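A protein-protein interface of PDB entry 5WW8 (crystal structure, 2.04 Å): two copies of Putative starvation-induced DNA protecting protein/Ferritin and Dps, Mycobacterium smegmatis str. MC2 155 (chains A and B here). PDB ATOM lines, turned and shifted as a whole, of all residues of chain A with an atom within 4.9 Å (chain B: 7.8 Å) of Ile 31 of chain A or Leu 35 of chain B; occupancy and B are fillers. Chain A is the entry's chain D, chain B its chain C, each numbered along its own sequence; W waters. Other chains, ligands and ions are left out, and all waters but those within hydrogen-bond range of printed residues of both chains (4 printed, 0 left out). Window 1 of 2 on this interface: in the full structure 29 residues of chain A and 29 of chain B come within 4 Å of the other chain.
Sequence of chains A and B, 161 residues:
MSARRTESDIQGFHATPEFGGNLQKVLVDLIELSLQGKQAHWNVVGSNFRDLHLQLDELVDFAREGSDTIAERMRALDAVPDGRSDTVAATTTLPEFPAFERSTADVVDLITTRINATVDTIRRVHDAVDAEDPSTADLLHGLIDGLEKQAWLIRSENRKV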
ATOM      1  N   LEU A  27       9.324  -1.976   8.742  1.00  0.00           N
ATOM      2  CA  LEU A  27      10.589  -1.278   8.957  1.00  0.00           C
ATOM      3  C   LEU A  27      10.582   0.154   8.429  1.00  0.00           C
ATOM      4  O   LEU A  27      10.907   1.075   9.185  1.00  0.00           O
ATOM      5  CB  LEU A  27      11.765  -2.066   8.366  1.00  0.00           C
ATOM      6  CG  LEU A  27      13.155  -1.445   8.556  1.00  0.00           C
ATOM      7  CD1 LEU A  27      13.577  -1.437  10.025  1.00  0.00           C
ATOM      8  CD2 LEU A  27      14.185  -2.159   7.707  1.00  0.00           C
ATOM      9  N   VAL A  28      10.191   0.338   7.155  1.00  0.00           N
ATOM     10  CA  VAL A  28      10.210   1.674   6.528  1.00  0.00           C
ATOM     11  C   VAL A  28       9.255   2.665   7.201  1.00  0.00           C
ATOM     12  O   VAL A  28       9.594   3.826   7.362  1.00  0.00           O
ATOM     13  CB  VAL A  28      10.019   1.653   4.984  1.00  0.00           C
ATOM     14  CG1 VAL A  28      11.229   1.010   4.316  1.00  0.00           C
ATOM     15  CG2 VAL A  28       8.721   0.952   4.571  1.00  0.00           C
ATOM     16  N   ASP A  29       8.085   2.193   7.620  1.00  0.00           N
ATOM     17  CA  ASP A  29       7.128   3.048   8.316  1.00  0.00           C
ATOM     18  C   ASP A  29       7.589   3.408   9.735  1.00  0.00           C
ATOM     19  O   ASP A  29       7.364   4.540  10.181  1.00  0.00           O
ATOM     20  CB  ASP A  29       5.728   2.442   8.303  1.00  0.00           C
ATOM     21  CG  ASP A  29       5.065   2.516   6.925  1.00  0.00           C
ATOM     22  OD1 ASP A  29       5.625   3.135   6.000  1.00  0.00           O
ATOM     23  OD2 ASP A  29       3.960   1.955   6.775  1.00  0.00           O
ATOM     24  N   LEU A  30       8.264   2.471  10.409  1.00  0.00           N
ATOM     25  CA  LEU A  30       8.892   2.767  11.709  1.00  0.00           C
ATOM     26  C   LEU A  30       9.997   3.822  11.597  1.00  0.00           C
ATOM     27  O   LEU A  30      10.029   4.775  12.392  1.00  0.00           O
ATOM     28  CB  LEU A  30       9.405   1.498  12.413  1.00  0.00           C
ATOM     29  CG  LEU A  30       8.355   0.573  13.034  1.00  0.00           C
ATOM     30  CD1 LEU A  30       8.999  -0.758  13.409  1.00  0.00           C
ATOM     31  CD2 LEU A  30       7.657   1.218  14.231  1.00  0.00           C
ATOM     32  N   ILE A  31      10.879   3.659  10.606  1.00  0.00           N
ATOM     33  CA  ILE A  31      11.937   4.647  10.344  1.00  0.00           C
ATOM     34  C   ILE A  31      11.357   6.004   9.942  1.00  0.00           C
ATOM     35  O   ILE A  31      11.778   7.031  10.473  1.00  0.00           O
ATOM     36  CB  ILE A  31      12.989   4.148   9.316  1.00  0.00           C
ATOM     37  CG1 ILE A  31      13.688   2.900   9.857  1.00  0.00           C
ATOM     38  CG2 ILE A  31      14.013   5.243   9.010  1.00  0.00           C
ATOM     39  CD1 ILE A  31      14.482   2.127   8.834  1.00  0.00           C
ATOM     40  N   GLU A  32      10.375   6.007   9.036  1.00  0.00           N
ATOM     41  CA  GLU A  32       9.709   7.255   8.640  1.00  0.00           C
ATOM     42  C   GLU A  32       9.057   7.955   9.838  1.00  0.00           C
ATOM     43  O   GLU A  32       9.191   9.184  10.008  1.00  0.00           O
ATOM     44  CB  GLU A  32       8.689   7.014   7.513  1.00  0.00           C
ATOM     45  CG  GLU A  32       7.912   8.248   7.054  1.00  0.00           C
ATOM     46  CD  GLU A  32       8.762   9.301   6.354  1.00  0.00           C
ATOM     47  OE1 GLU A  32       8.215  10.382   6.078  1.00  0.00           O
ATOM     48  OE2 GLU A  32       9.960   9.061   6.072  1.00  0.00           O
ATOM     49  N   LEU A  33       8.382   7.167  10.672  1.00  0.00           N
ATOM     50  CA  LEU A  33       7.810   7.669  11.907  1.00  0.00           C
ATOM     51  C   LEU A  33       8.847   8.344  12.817  1.00  0.00           C
ATOM     52  O   LEU A  33       8.565   9.429  13.344  1.00  0.00           O
ATOM     53  CB  LEU A  33       7.037   6.572  12.652  1.00  0.00           C
ATOM     54  CG  LEU A  33       6.234   6.963  13.896  1.00  0.00           C
ATOM     55  CD1 LEU A  33       5.167   8.021  13.595  1.00  0.00           C
ATOM     56  CD2 LEU A  33       5.619   5.723  14.522  1.00  0.00           C
ATOM     57  N   SER A  34      10.027   7.726  12.973  1.00  0.00           N
ATOM     58  CA  SER A  34      11.133   8.284  13.787  1.00  0.00           C
ATOM     59  C   SER A  34      11.604   9.625  13.233  1.00  0.00           C
ATOM     60  O   SER A  34      11.860  10.583  13.983  1.00  0.00           O
ATOM     61  CB  SER A  34      12.327   7.325  13.828  1.00  0.00           C
ATOM     62  OG  SER A  34      11.972   6.063  14.351  1.00  0.00           O
ATOM     63  N   LEU A  35      11.725   9.684  11.902  1.00  0.00           N
ATOM     64  CA  LEU A  35      12.164  10.903  11.212  1.00  0.00           C
ATOM     65  C   LEU A  35      11.136  12.028  11.341  1.00  0.00           C
ATOM     66  O   LEU A  35      11.493  13.171  11.611  1.00  0.00           O
ATOM     67  CB  LEU A  35      12.514  10.611   9.739  1.00  0.00           C
ATOM     68  CG  LEU A  35      13.731   9.710   9.452  1.00  0.00           C
ATOM     69  CD1 LEU A  35      13.774   9.312   7.985  1.00  0.00           C
ATOM     70  CD2 LEU A  35      15.056  10.346   9.873  1.00  0.00           C
ATOM     71  N   SER A  67      12.329  -0.279  15.035  1.00  0.00           N
ATOM     72  CA  SER A  67      12.980  -0.508  13.742  1.00  0.00           C
ATOM     73  C   SER A  67      14.215  -1.392  13.877  1.00  0.00           C
ATOM     74  O   SER A  67      14.440  -2.250  13.035  1.00  0.00           O
ATOM     75  CB  SER A  67      13.320   0.804  13.032  1.00  0.00           C
ATOM     76  OG  SER A  67      14.123   1.624  13.851  1.00  0.00           O
ATOM     77  N   GLY A  83      16.866   0.139   5.348  1.00  0.00           N
ATOM     78  CA  GLY A  83      16.458   1.382   6.007  1.00  0.00           C
ATOM     79  C   GLY A  83      17.099   2.669   5.492  1.00  0.00           C
ATOM     80  O   GLY A  83      17.126   3.677   6.206  1.00  0.00           O
ATOM     81  N   SER A  85      17.648   6.165   3.388  1.00  0.00           N
ATOM     82  CA  SER A  85      16.743   7.320   3.197  1.00  0.00           C
ATOM     83  C   SER A  85      15.888   7.247   1.923  1.00  0.00           C
ATOM     84  O   SER A  85      14.676   7.432   2.004  1.00  0.00           O
ATOM     85  CB  SER A  85      17.505   8.645   3.239  1.00  0.00           C
ATOM     86  OG  SER A  85      18.540   8.660   2.269  1.00  0.00           O
ATOM     87  N   VAL A  88      13.214   4.537   2.277  1.00  0.00           N
ATOM     88  CA  VAL A  88      12.179   4.972   3.229  1.00  0.00           C
ATOM     89  C   VAL A  88      11.256   6.021   2.578  1.00  0.00           C
ATOM     90  O   VAL A  88      10.039   5.875   2.617  1.00  0.00           O
ATOM     91  CB  VAL A  88      12.771   5.469   4.585  1.00  0.00           C
ATOM     92  CG1 VAL A  88      11.689   6.064   5.470  1.00  0.00           C
ATOM     93  CG2 VAL A  88      13.488   4.333   5.321  1.00  0.00           C
ATOM     94  N   VAL B  28      21.604  17.317   7.472  1.00  0.00           N
ATOM     95  CA  VAL B  28      21.156  16.254   6.555  1.00  0.00           C
ATOM     96  C   VAL B  28      22.216  15.181   6.397  1.00  0.00           C
ATOM     97  O   VAL B  28      21.881  14.012   6.226  1.00  0.00           O
ATOM     98  CB  VAL B  28      20.666  16.757   5.161  1.00  0.00           C
ATOM     99  CG1 VAL B  28      19.437  17.642   5.318  1.00  0.00           C
ATOM    100  CG2 VAL B  28      21.764  17.469   4.372  1.00  0.00           C
ATOM    101  N   ASP B  29      23.483  15.585   6.478  1.00  0.00           N
ATOM    102  CA  ASP B  29      24.577  14.642   6.365  1.00  0.00           C
ATOM    103  C   ASP B  29      24.728  13.819   7.639  1.00  0.00           C
ATOM    104  O   ASP B  29      25.057  12.635   7.570  1.00  0.00           O
ATOM    105  CB  ASP B  29      25.881  15.334   5.925  1.00  0.00           C
ATOM    106  CG  ASP B  29      25.876  15.696   4.435  1.00  0.00           C
ATOM    107  OD1 ASP B  29      24.964  15.241   3.700  1.00  0.00           O
ATOM    108  OD2 ASP B  29      26.788  16.426   3.989  1.00  0.00           O
ATOM    109  N   LEU B  30      24.434  14.427   8.787  1.00  0.00           N
ATOM    110  CA  LEU B  30      24.394  13.678  10.060  1.00  0.00           C
ATOM    111  C   LEU B  30      23.262  12.632  10.111  1.00  0.00           C
ATOM    112  O   LEU B  30      23.474  11.495  10.578  1.00  0.00           O
ATOM    113  CB  LEU B  30      24.316  14.632  11.260  1.00  0.00           C
ATOM    114  CG  LEU B  30      25.560  15.460  11.617  1.00  0.00           C
ATOM    115  CD1 LEU B  30      25.196  16.497  12.671  1.00  0.00           C
ATOM    116  CD2 LEU B  30      26.715  14.586  12.104  1.00  0.00           C
ATOM    117  N   ILE B  31      22.073  13.017   9.638  1.00  0.00           N
ATOM    118  CA  ILE B  31      20.930  12.097   9.589  1.00  0.00           C
ATOM    119  C   ILE B  31      21.213  10.958   8.603  1.00  0.00           C
ATOM    120  O   ILE B  31      20.980   9.785   8.924  1.00  0.00           O
ATOM    121  CB  ILE B  31      19.597  12.804   9.251  1.00  0.00           C
ATOM    122  CG1 ILE B  31      19.213  13.795  10.359  1.00  0.00           C
ATOM    123  CG2 ILE B  31      18.484  11.780   9.051  1.00  0.00           C
ATOM    124  CD1 ILE B  31      18.213  14.852   9.926  1.00  0.00           C
ATOM    125  N   GLU B  32      21.738  11.309   7.424  1.00  0.00           N
ATOM    126  CA  GLU B  32      22.107  10.313   6.421  1.00  0.00           C
ATOM    127  C   GLU B  32      23.142   9.332   6.974  1.00  0.00           C
ATOM    128  O   GLU B  32      22.998   8.118   6.795  1.00  0.00           O
ATOM    129  CB  GLU B  32      22.595  10.980   5.123  1.00  0.00           C
ATOM    130  CG  GLU B  32      22.963  10.037   3.983  1.00  0.00           C
ATOM    131  CD  GLU B  32      21.806   9.205   3.428  1.00  0.00           C
ATOM    132  OE1 GLU B  32      20.622   9.439   3.771  1.00  0.00           O
ATOM    133  OE2 GLU B  32      22.095   8.292   2.624  1.00  0.00           O
ATOM    134  N   LEU B  33      24.173   9.856   7.642  1.00  0.00           N
ATOM    135  CA  LEU B  33      25.185   9.014   8.284  1.00  0.00           C
ATOM    136  C   LEU B  33      24.561   8.034   9.292  1.00  0.00           C
ATOM    137  O   LEU B  33      24.902   6.840   9.278  1.00  0.00           O
ATOM    138  CB  LEU B  33      26.291   9.862   8.943  1.00  0.00           C
ATOM    139  CG  LEU B  33      27.539   9.117   9.455  1.00  0.00           C
ATOM    140  CD1 LEU B  33      28.264   8.358   8.349  1.00  0.00           C
ATOM    141  CD2 LEU B  33      28.489  10.094  10.136  1.00  0.00           C
ATOM    142  N   SER B  34      23.651   8.547  10.134  1.00  0.00           N
ATOM    143  CA  SER B  34      22.902   7.740  11.107  1.00  0.00           C
ATOM    144  C   SER B  34      22.133   6.596  10.440  1.00  0.00           C
ATOM    145  O   SER B  34      22.143   5.461  10.927  1.00  0.00           O
ATOM    146  CB  SER B  34      21.910   8.604  11.890  1.00  0.00           C
ATOM    147  OG  SER B  34      22.541   9.707  12.502  1.00  0.00           O
ATOM    148  N   LEU B  35      21.446   6.916   9.336  1.00  0.00           N
ATOM    149  CA  LEU B  35      20.663   5.916   8.595  1.00  0.00           C
ATOM    150  C   LEU B  35      21.583   4.904   7.917  1.00  0.00           C
ATOM    151  O   LEU B  35      21.323   3.696   7.961  1.00  0.00           O
ATOM    152  CB  LEU B  35      19.706   6.571   7.580  1.00  0.00           C
ATOM    153  CG  LEU B  35      18.580   7.474   8.111  1.00  0.00           C
ATOM    154  CD1 LEU B  35      18.043   8.356   6.998  1.00  0.00           C
ATOM    155  CD2 LEU B  35      17.441   6.699   8.773  1.00  0.00           C
ATOM    156  N   GLN B  36      22.665   5.396   7.315  1.00  0.00           N
ATOM    157  CA  GLN B  36      23.652   4.524   6.677  1.00  0.00           C
ATOM    158  C   GLN B  36      24.365   3.629   7.699  1.00  0.00           C
ATOM    159  O   GLN B  36      24.578   2.441   7.448  1.00  0.00           O
ATOM    160  CB  GLN B  36      24.658   5.341   5.862  1.00  0.00           C
ATOM    161  CG  GLN B  36      24.062   5.991   4.615  1.00  0.00           C
ATOM    162  CD  GLN B  36      25.131   6.551   3.695  1.00  0.00           C
ATOM    163  OE1 GLN B  36      26.310   6.316   3.911  1.00  0.00           O
ATOM    164  NE2 GLN B  36      24.728   7.302   2.678  1.00  0.00           N
ATOM    165  N   GLY B  37      24.711   4.210   8.846  1.00  0.00           N
ATOM    166  CA  GLY B  37      25.302   3.469   9.954  1.00  0.00           C
ATOM    167  C   GLY B  37      24.430   2.317  10.437  1.00  0.00           C
ATOM    168  O   GLY B  37      24.952   1.219  10.673  1.00  0.00           O
ATOM    169  N   LYS B  38      23.120   2.554  10.585  1.00  0.00           N
ATOM    170  CA  LYS B  38      22.198   1.472  10.979  1.00  0.00           C
ATOM    171  C   LYS B  38      22.098   0.400   9.903  1.00  0.00           C
ATOM    172  O   LYS B  38      22.116  -0.791  10.218  1.00  0.00           O
ATOM    173  CB  LYS B  38      20.797   1.982  11.351  1.00  0.00           C
ATOM    174  CG  LYS B  38      20.696   2.625  12.730  1.00  0.00           C
ATOM    175  CD  LYS B  38      21.247   1.732  13.842  1.00  0.00           C
ATOM    176  CE  LYS B  38      20.152   1.118  14.671  1.00  0.00           C
ATOM    177  NZ  LYS B  38      20.698   0.438  15.883  1.00  0.00           N
ATOM    178  N   GLN B  39      22.021   0.834   8.643  1.00  0.00           N
ATOM    179  CA  GLN B  39      22.019  -0.083   7.500  1.00  0.00           C
ATOM    180  C   GLN B  39      23.246  -1.011   7.550  1.00  0.00           C
ATOM    181  O   GLN B  39      23.091  -2.231   7.462  1.00  0.00           O
ATOM    182  CB  GLN B  39      21.947   0.702   6.171  1.00  0.00           C
ATOM    183  CG  GLN B  39      21.920  -0.143   4.894  1.00  0.00           C
ATOM    184  CD  GLN B  39      20.587  -0.841   4.628  1.00  0.00           C
ATOM    185  OE1 GLN B  39      19.563  -0.551   5.258  1.00  0.00           O
ATOM    186  NE2 GLN B  39      20.598  -1.771   3.673  1.00  0.00           N
ATOM    187  N   ALA B  40      24.440  -0.418   7.713  1.00  0.00           N
ATOM    188  CA  ALA B  40      25.709  -1.154   7.865  1.00  0.00           C
ATOM    189  C   ALA B  40      25.688  -2.086   9.088  1.00  0.00           C
ATOM    190  O   ALA B  40      26.042  -3.267   8.981  1.00  0.00           O
ATOM    191  CB  ALA B  40      26.892  -0.197   7.941  1.00  0.00           C
ATOM    192  N   HIS B  41      25.253  -1.538  10.226  1.00  0.00           N
ATOM    193  CA  HIS B  41      25.103  -2.274  11.497  1.00  0.00           C
ATOM    194  C   HIS B  41      24.311  -3.591  11.319  1.00  0.00           C
ATOM    195  O   HIS B  41      24.760  -4.658  11.767  1.00  0.00           O
ATOM    196  CB  HIS B  41      24.446  -1.341  12.524  1.00  0.00           C
ATOM    197  CG  HIS B  41      24.032  -2.002  13.800  1.00  0.00           C
ATOM    198  ND1 HIS B  41      24.918  -2.263  14.827  1.00  0.00           N
ATOM    199  CD2 HIS B  41      22.818  -2.408  14.237  1.00  0.00           C
ATOM    200  CE1 HIS B  41      24.268  -2.817  15.835  1.00  0.00           C
ATOM    201  NE2 HIS B  41      22.993  -2.910  15.504  1.00  0.00           N
ATOM    202  N   TRP B  42      23.168  -3.517  10.634  1.00  0.00           N
ATOM    203  CA  TRP B  42      22.333  -4.696  10.378  1.00  0.00           C
ATOM    204  C   TRP B  42      22.938  -5.680   9.384  1.00  0.00           C
ATOM    205  O   TRP B  42      22.876  -6.895   9.602  1.00  0.00           O
ATOM    206  CB  TRP B  42      20.939  -4.298   9.879  1.00  0.00           C
ATOM    207  CG  TRP B  42      20.157  -3.405  10.814  1.00  0.00           C
ATOM    208  CD1 TRP B  42      20.086  -3.492  12.180  1.00  0.00           C
ATOM    209  CD2 TRP B  42      19.309  -2.315  10.435  1.00  0.00           C
ATOM    210  NE1 TRP B  42      19.255  -2.509  12.677  1.00  0.00           N
ATOM    211  CE2 TRP B  42      18.767  -1.769  11.630  1.00  0.00           C
ATOM    212  CE3 TRP B  42      18.949  -1.747   9.200  1.00  0.00           C
ATOM    213  CZ2 TRP B  42      17.882  -0.681  11.628  1.00  0.00           C
ATOM    214  CZ3 TRP B  42      18.078  -0.655   9.195  1.00  0.00           C
ATOM    215  CH2 TRP B  42      17.556  -0.131  10.406  1.00  0.00           C
ATOM    216  N   VAL B  60      26.312   5.530  15.179  1.00  0.00           N
ATOM    217  CA  VAL B  60      24.921   5.950  15.014  1.00  0.00           C
ATOM    218  C   VAL B  60      24.465   6.817  16.197  1.00  0.00           C
ATOM    219  O   VAL B  60      23.851   7.872  15.983  1.00  0.00           O
ATOM    220  CB  VAL B  60      23.994   4.746  14.762  1.00  0.00           C
ATOM    221  CG1 VAL B  60      22.531   5.160  14.785  1.00  0.00           C
ATOM    222  CG2 VAL B  60      24.328   4.137  13.407  1.00  0.00           C
ATOM    223  N   ALA B  63      26.047  10.191  15.841  1.00  0.00           N
ATOM    224  CA  ALA B  63      25.465  10.936  14.727  1.00  0.00           C
ATOM    225  C   ALA B  63      24.051  11.433  15.035  1.00  0.00           C
ATOM    226  O   ALA B  63      23.718  12.566  14.683  1.00  0.00           O
ATOM    227  CB  ALA B  63      25.516  10.125  13.438  1.00  0.00           C
ATOM    228  N   ARG B  64      23.251  10.607  15.722  1.00  0.00           N
ATOM    229  CA  ARG B  64      21.897  10.988  16.190  1.00  0.00           C
ATOM    230  C   ARG B  64      21.915  12.094  17.242  1.00  0.00           C
ATOM    231  O   ARG B  64      21.124  13.038  17.156  1.00  0.00           O
ATOM    232  CB  ARG B  64      21.139   9.787  16.757  1.00  0.00           C
ATOM    233  CG  ARG B  64      20.608   8.820  15.710  1.00  0.00           C
ATOM    234  CD  ARG B  64      19.989   7.621  16.404  1.00  0.00           C
ATOM    235  NE  ARG B  64      19.395   6.690  15.446  1.00  0.00           N
ATOM    236  CZ  ARG B  64      18.990   5.454  15.741  1.00  0.00           C
ATOM    237  NH1 ARG B  64      19.103   4.980  16.973  1.00  0.00           N
ATOM    238  NH2 ARG B  64      18.467   4.691  14.798  1.00  0.00           N
ATOM    239  N   GLY B  83      14.681  17.715   8.678  1.00  0.00           N
ATOM    240  CA  GLY B  83      15.248  16.376   8.745  1.00  0.00           C
ATOM    241  C   GLY B  83      14.389  15.281   8.127  1.00  0.00           C
ATOM    242  O   GLY B  83      14.612  14.099   8.404  1.00  0.00           O
ATOM    243  N   ARG B  84      13.417  15.664   7.295  1.00  0.00           N
ATOM    244  CA  ARG B  84      12.495  14.691   6.681  1.00  0.00           C
ATOM    245  C   ARG B  84      13.203  13.810   5.649  1.00  0.00           C
ATOM    246  O   ARG B  84      14.205  14.227   5.051  1.00  0.00           O
ATOM    247  CB  ARG B  84      11.279  15.386   6.061  1.00  0.00           C
ATOM    248  CG  ARG B  84      10.397  16.097   7.079  1.00  0.00           C
ATOM    249  CD  ARG B  84       9.347  16.962   6.392  1.00  0.00           C
ATOM    250  NE  ARG B  84       9.924  17.990   5.522  1.00  0.00           N
ATOM    251  CZ  ARG B  84       9.254  18.663   4.584  1.00  0.00           C
ATOM    252  NH1 ARG B  84       7.965  18.425   4.373  1.00  0.00           N
ATOM    253  NH2 ARG B  84       9.883  19.574   3.848  1.00  0.00           N
ATOM    254  N   SER B  85      12.672  12.600   5.458  1.00  0.00           N
ATOM    255  CA  SER B  85      13.286  11.589   4.603  1.00  0.00           C
ATOM    256  C   SER B  85      13.562  12.060   3.173  1.00  0.00           C
ATOM    257  O   SER B  85      14.663  11.862   2.670  1.00  0.00           O
ATOM    258  CB  SER B  85      12.432  10.326   4.580  1.00  0.00           C
ATOM    259  OG  SER B  85      11.119  10.622   4.126  1.00  0.00           O
ATOM    260  N   VAL B  88      16.414  14.742   3.187  1.00  0.00           N
ATOM    261  CA  VAL B  88      17.696  14.083   3.461  1.00  0.00           C
ATOM    262  C   VAL B  88      18.181  13.365   2.188  1.00  0.00           C
ATOM    263  O   VAL B  88      19.296  13.609   1.744  1.00  0.00           O
ATOM    264  CB  VAL B  88      17.631  13.152   4.711  1.00  0.00           C
ATOM    265  CG1 VAL B  88      18.891  12.304   4.857  1.00  0.00           C
ATOM    266  CG2 VAL B  88      17.434  13.975   5.982  1.00  0.00           C
ATOM    267  N   ALA B  89      17.328  12.528   1.590  1.00  0.00           N
ATOM    268  CA  ALA B  89      17.674  11.820   0.339  1.00  0.00           C
ATOM    269  C   ALA B  89      18.032  12.780  -0.796  1.00  0.00           C
ATOM    270  O   ALA B  89      19.009  12.552  -1.512  1.00  0.00           O
ATOM    271  CB  ALA B  89      16.548  10.886  -0.089  1.00  0.00           C
ATOM    272  N   PHE B  97      24.934   4.537   0.408  1.00  0.00           N
ATOM    273  CA  PHE B  97      25.374   3.264   0.957  1.00  0.00           C
ATOM    274  C   PHE B  97      24.652   2.151   0.176  1.00  0.00           C
ATOM    275  O   PHE B  97      23.461   2.291  -0.136  1.00  0.00           O
ATOM    276  CB  PHE B  97      25.095   3.188   2.467  1.00  0.00           C
ATOM    277  CG  PHE B  97      25.784   2.037   3.159  1.00  0.00           C
ATOM    278  CD1 PHE B  97      27.086   2.171   3.644  1.00  0.00           C
ATOM    279  CD2 PHE B  97      25.133   0.806   3.309  1.00  0.00           C
ATOM    280  CE1 PHE B  97      27.722   1.101   4.264  1.00  0.00           C
ATOM    281  CE2 PHE B  97      25.758  -0.269   3.929  1.00  0.00           C
ATOM    282  CZ  PHE B  97      27.056  -0.121   4.407  1.00  0.00           C
ATOM    283  N   ILE B 111      31.975   2.940   5.176  1.00  0.00           N
ATOM    284  CA  ILE B 111      31.607   3.786   6.307  1.00  0.00           C
ATOM    285  C   ILE B 111      32.676   4.858   6.587  1.00  0.00           C
ATOM    286  O   ILE B 111      32.325   6.014   6.849  1.00  0.00           O
ATOM    287  CB  ILE B 111      31.200   2.936   7.550  1.00  0.00           C
ATOM    288  CG1 ILE B 111      29.827   2.250   7.315  1.00  0.00           C
ATOM    289  CG2 ILE B 111      31.177   3.755   8.838  1.00  0.00           C
ATOM    290  CD1 ILE B 111      28.608   3.181   7.236  1.00  0.00           C
HETATM  291  O   HOH W   1      20.440   6.062   4.107  1.00  0.00           O
HETATM  292  O   HOH W   2      18.623   3.016   8.557  1.00  0.00           O
HETATM  293  O   HOH W   3      14.321  13.835  11.240  1.00  0.00           O
HETATM  294  O   HOH W   4      10.255  12.126   7.189  1.00  0.00           O
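The side-chain amide nitrogen (NE2) of Gln 36 of chain B lies within hydrogen-bond range of the side-chain carboxylate (OE2) of Glu 32 of chain B, 2.8 Å away.
Leu 35 of chain B touches Ile 31 of chain A (CD2 to CG2, 3.7 Å). CG2 of Ile 31 of chain B touches CD2 of Leu 35 of chain A, 3.8 Å away. Ser 85 of chain B touches Leu 35 of chain A (CB to CD1, 3.8 Å). Gly 83 of chain A touches Leu 35 of chain B. CD1 of Leu 35 of chain B touches CB of Ser 85 of chain A, at 3.8 Å. Ala 89 of chain B touches Ser 85 of chain A.
Ser 34 of chain A touches none of the printed residues of chain B. Printed residues of chain B within 4 Å of Ser 85 of chain A: Glu 32 (2.7 Å), Leu 35 (3.8 Å) and Ala 89 (3.8 Å). Leu 35 of chain B touches just these residues of chain A: Ile 31, Gly 83 and Ser 85. Of the printed residues of chain A, Gln 39 of chain B touches Gly 83 (2.8 Å). The nearest printed residue of chain B that does not touch Glu 32 of chain A is Arg 84 of chain B (5.8 Å).
The side-chain carboxylate (OE1) of Glu 32 of chain B lies within hydrogen-bond range of the side-chain hydroxyl (OG) of Ser 85 of chain A (2.7 Å). The backbone NH of Gly 83 of chain A is in hydrogen-bond range of the side-chain amide oxygen of Gln 39 of chain B, 2.8 Å away. The side-chain hydroxyl (OG) of Ser 85 of chain B sits at hydrogen-bond distance from the side-chain carboxylate (OE2) of Glu 32 of chain A, 2.8 Å away.
Water W2 lies within hydrogen-bond range of O of Leu 35 of chain B (2.8 Å) and O of Gly 83 of chain A (2.9 Å). Water W3 bridges O of Gly 83 of chain B (2.9 Å) and O of Leu 35 of chain A (2.9 Å). Water W1 bridges the backbone NH of Ser 85 of chain A (2.9 Å) and the side-chain carboxylate of Glu 32 of chain B (3.1 Å). Water W4 bridges OE1 of Glu 32 of chain A and N of Ser 85 of chain B.
Ile 31 of chain A touches Leu 35 of chain B, and with the chains exchanged Leu 35 of chain A touches Ile 31 of chain B. Glu 32 of chain A touches Ser 85 of chain B, and with the chains exchanged Ser 85 of chain A touches Glu 32 of chain B. Leu 35 of chain A touches Ser 85 of chain B, and with the chains exchanged Ser 85 of chain A touches Leu 35 of chain B. Gly 83 of chain A touches Leu 35 of chain B, but with the chains exchanged Leu 35 of chain A does not touch Gly 83 of chain B (4.1 Å). Of the 9 pairs that touch across the chains among the printed residues, 6 have their exchanged pair printed and touching as well.
Of the 13 printed residues of chain A, 5 touch a printed residue of chain B. Printed residues of chain A that touch a printed residue of chain B: Ile 31, Glu 32, Leu 35, Gly 83 and Ser 85. Among the printed residues, 9 pairs touch across the chains. Among the printed residues, no Asp or Glu carboxylate lies within 4 Å of a Lys or Arg side-chain nitrogen of the other chain.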
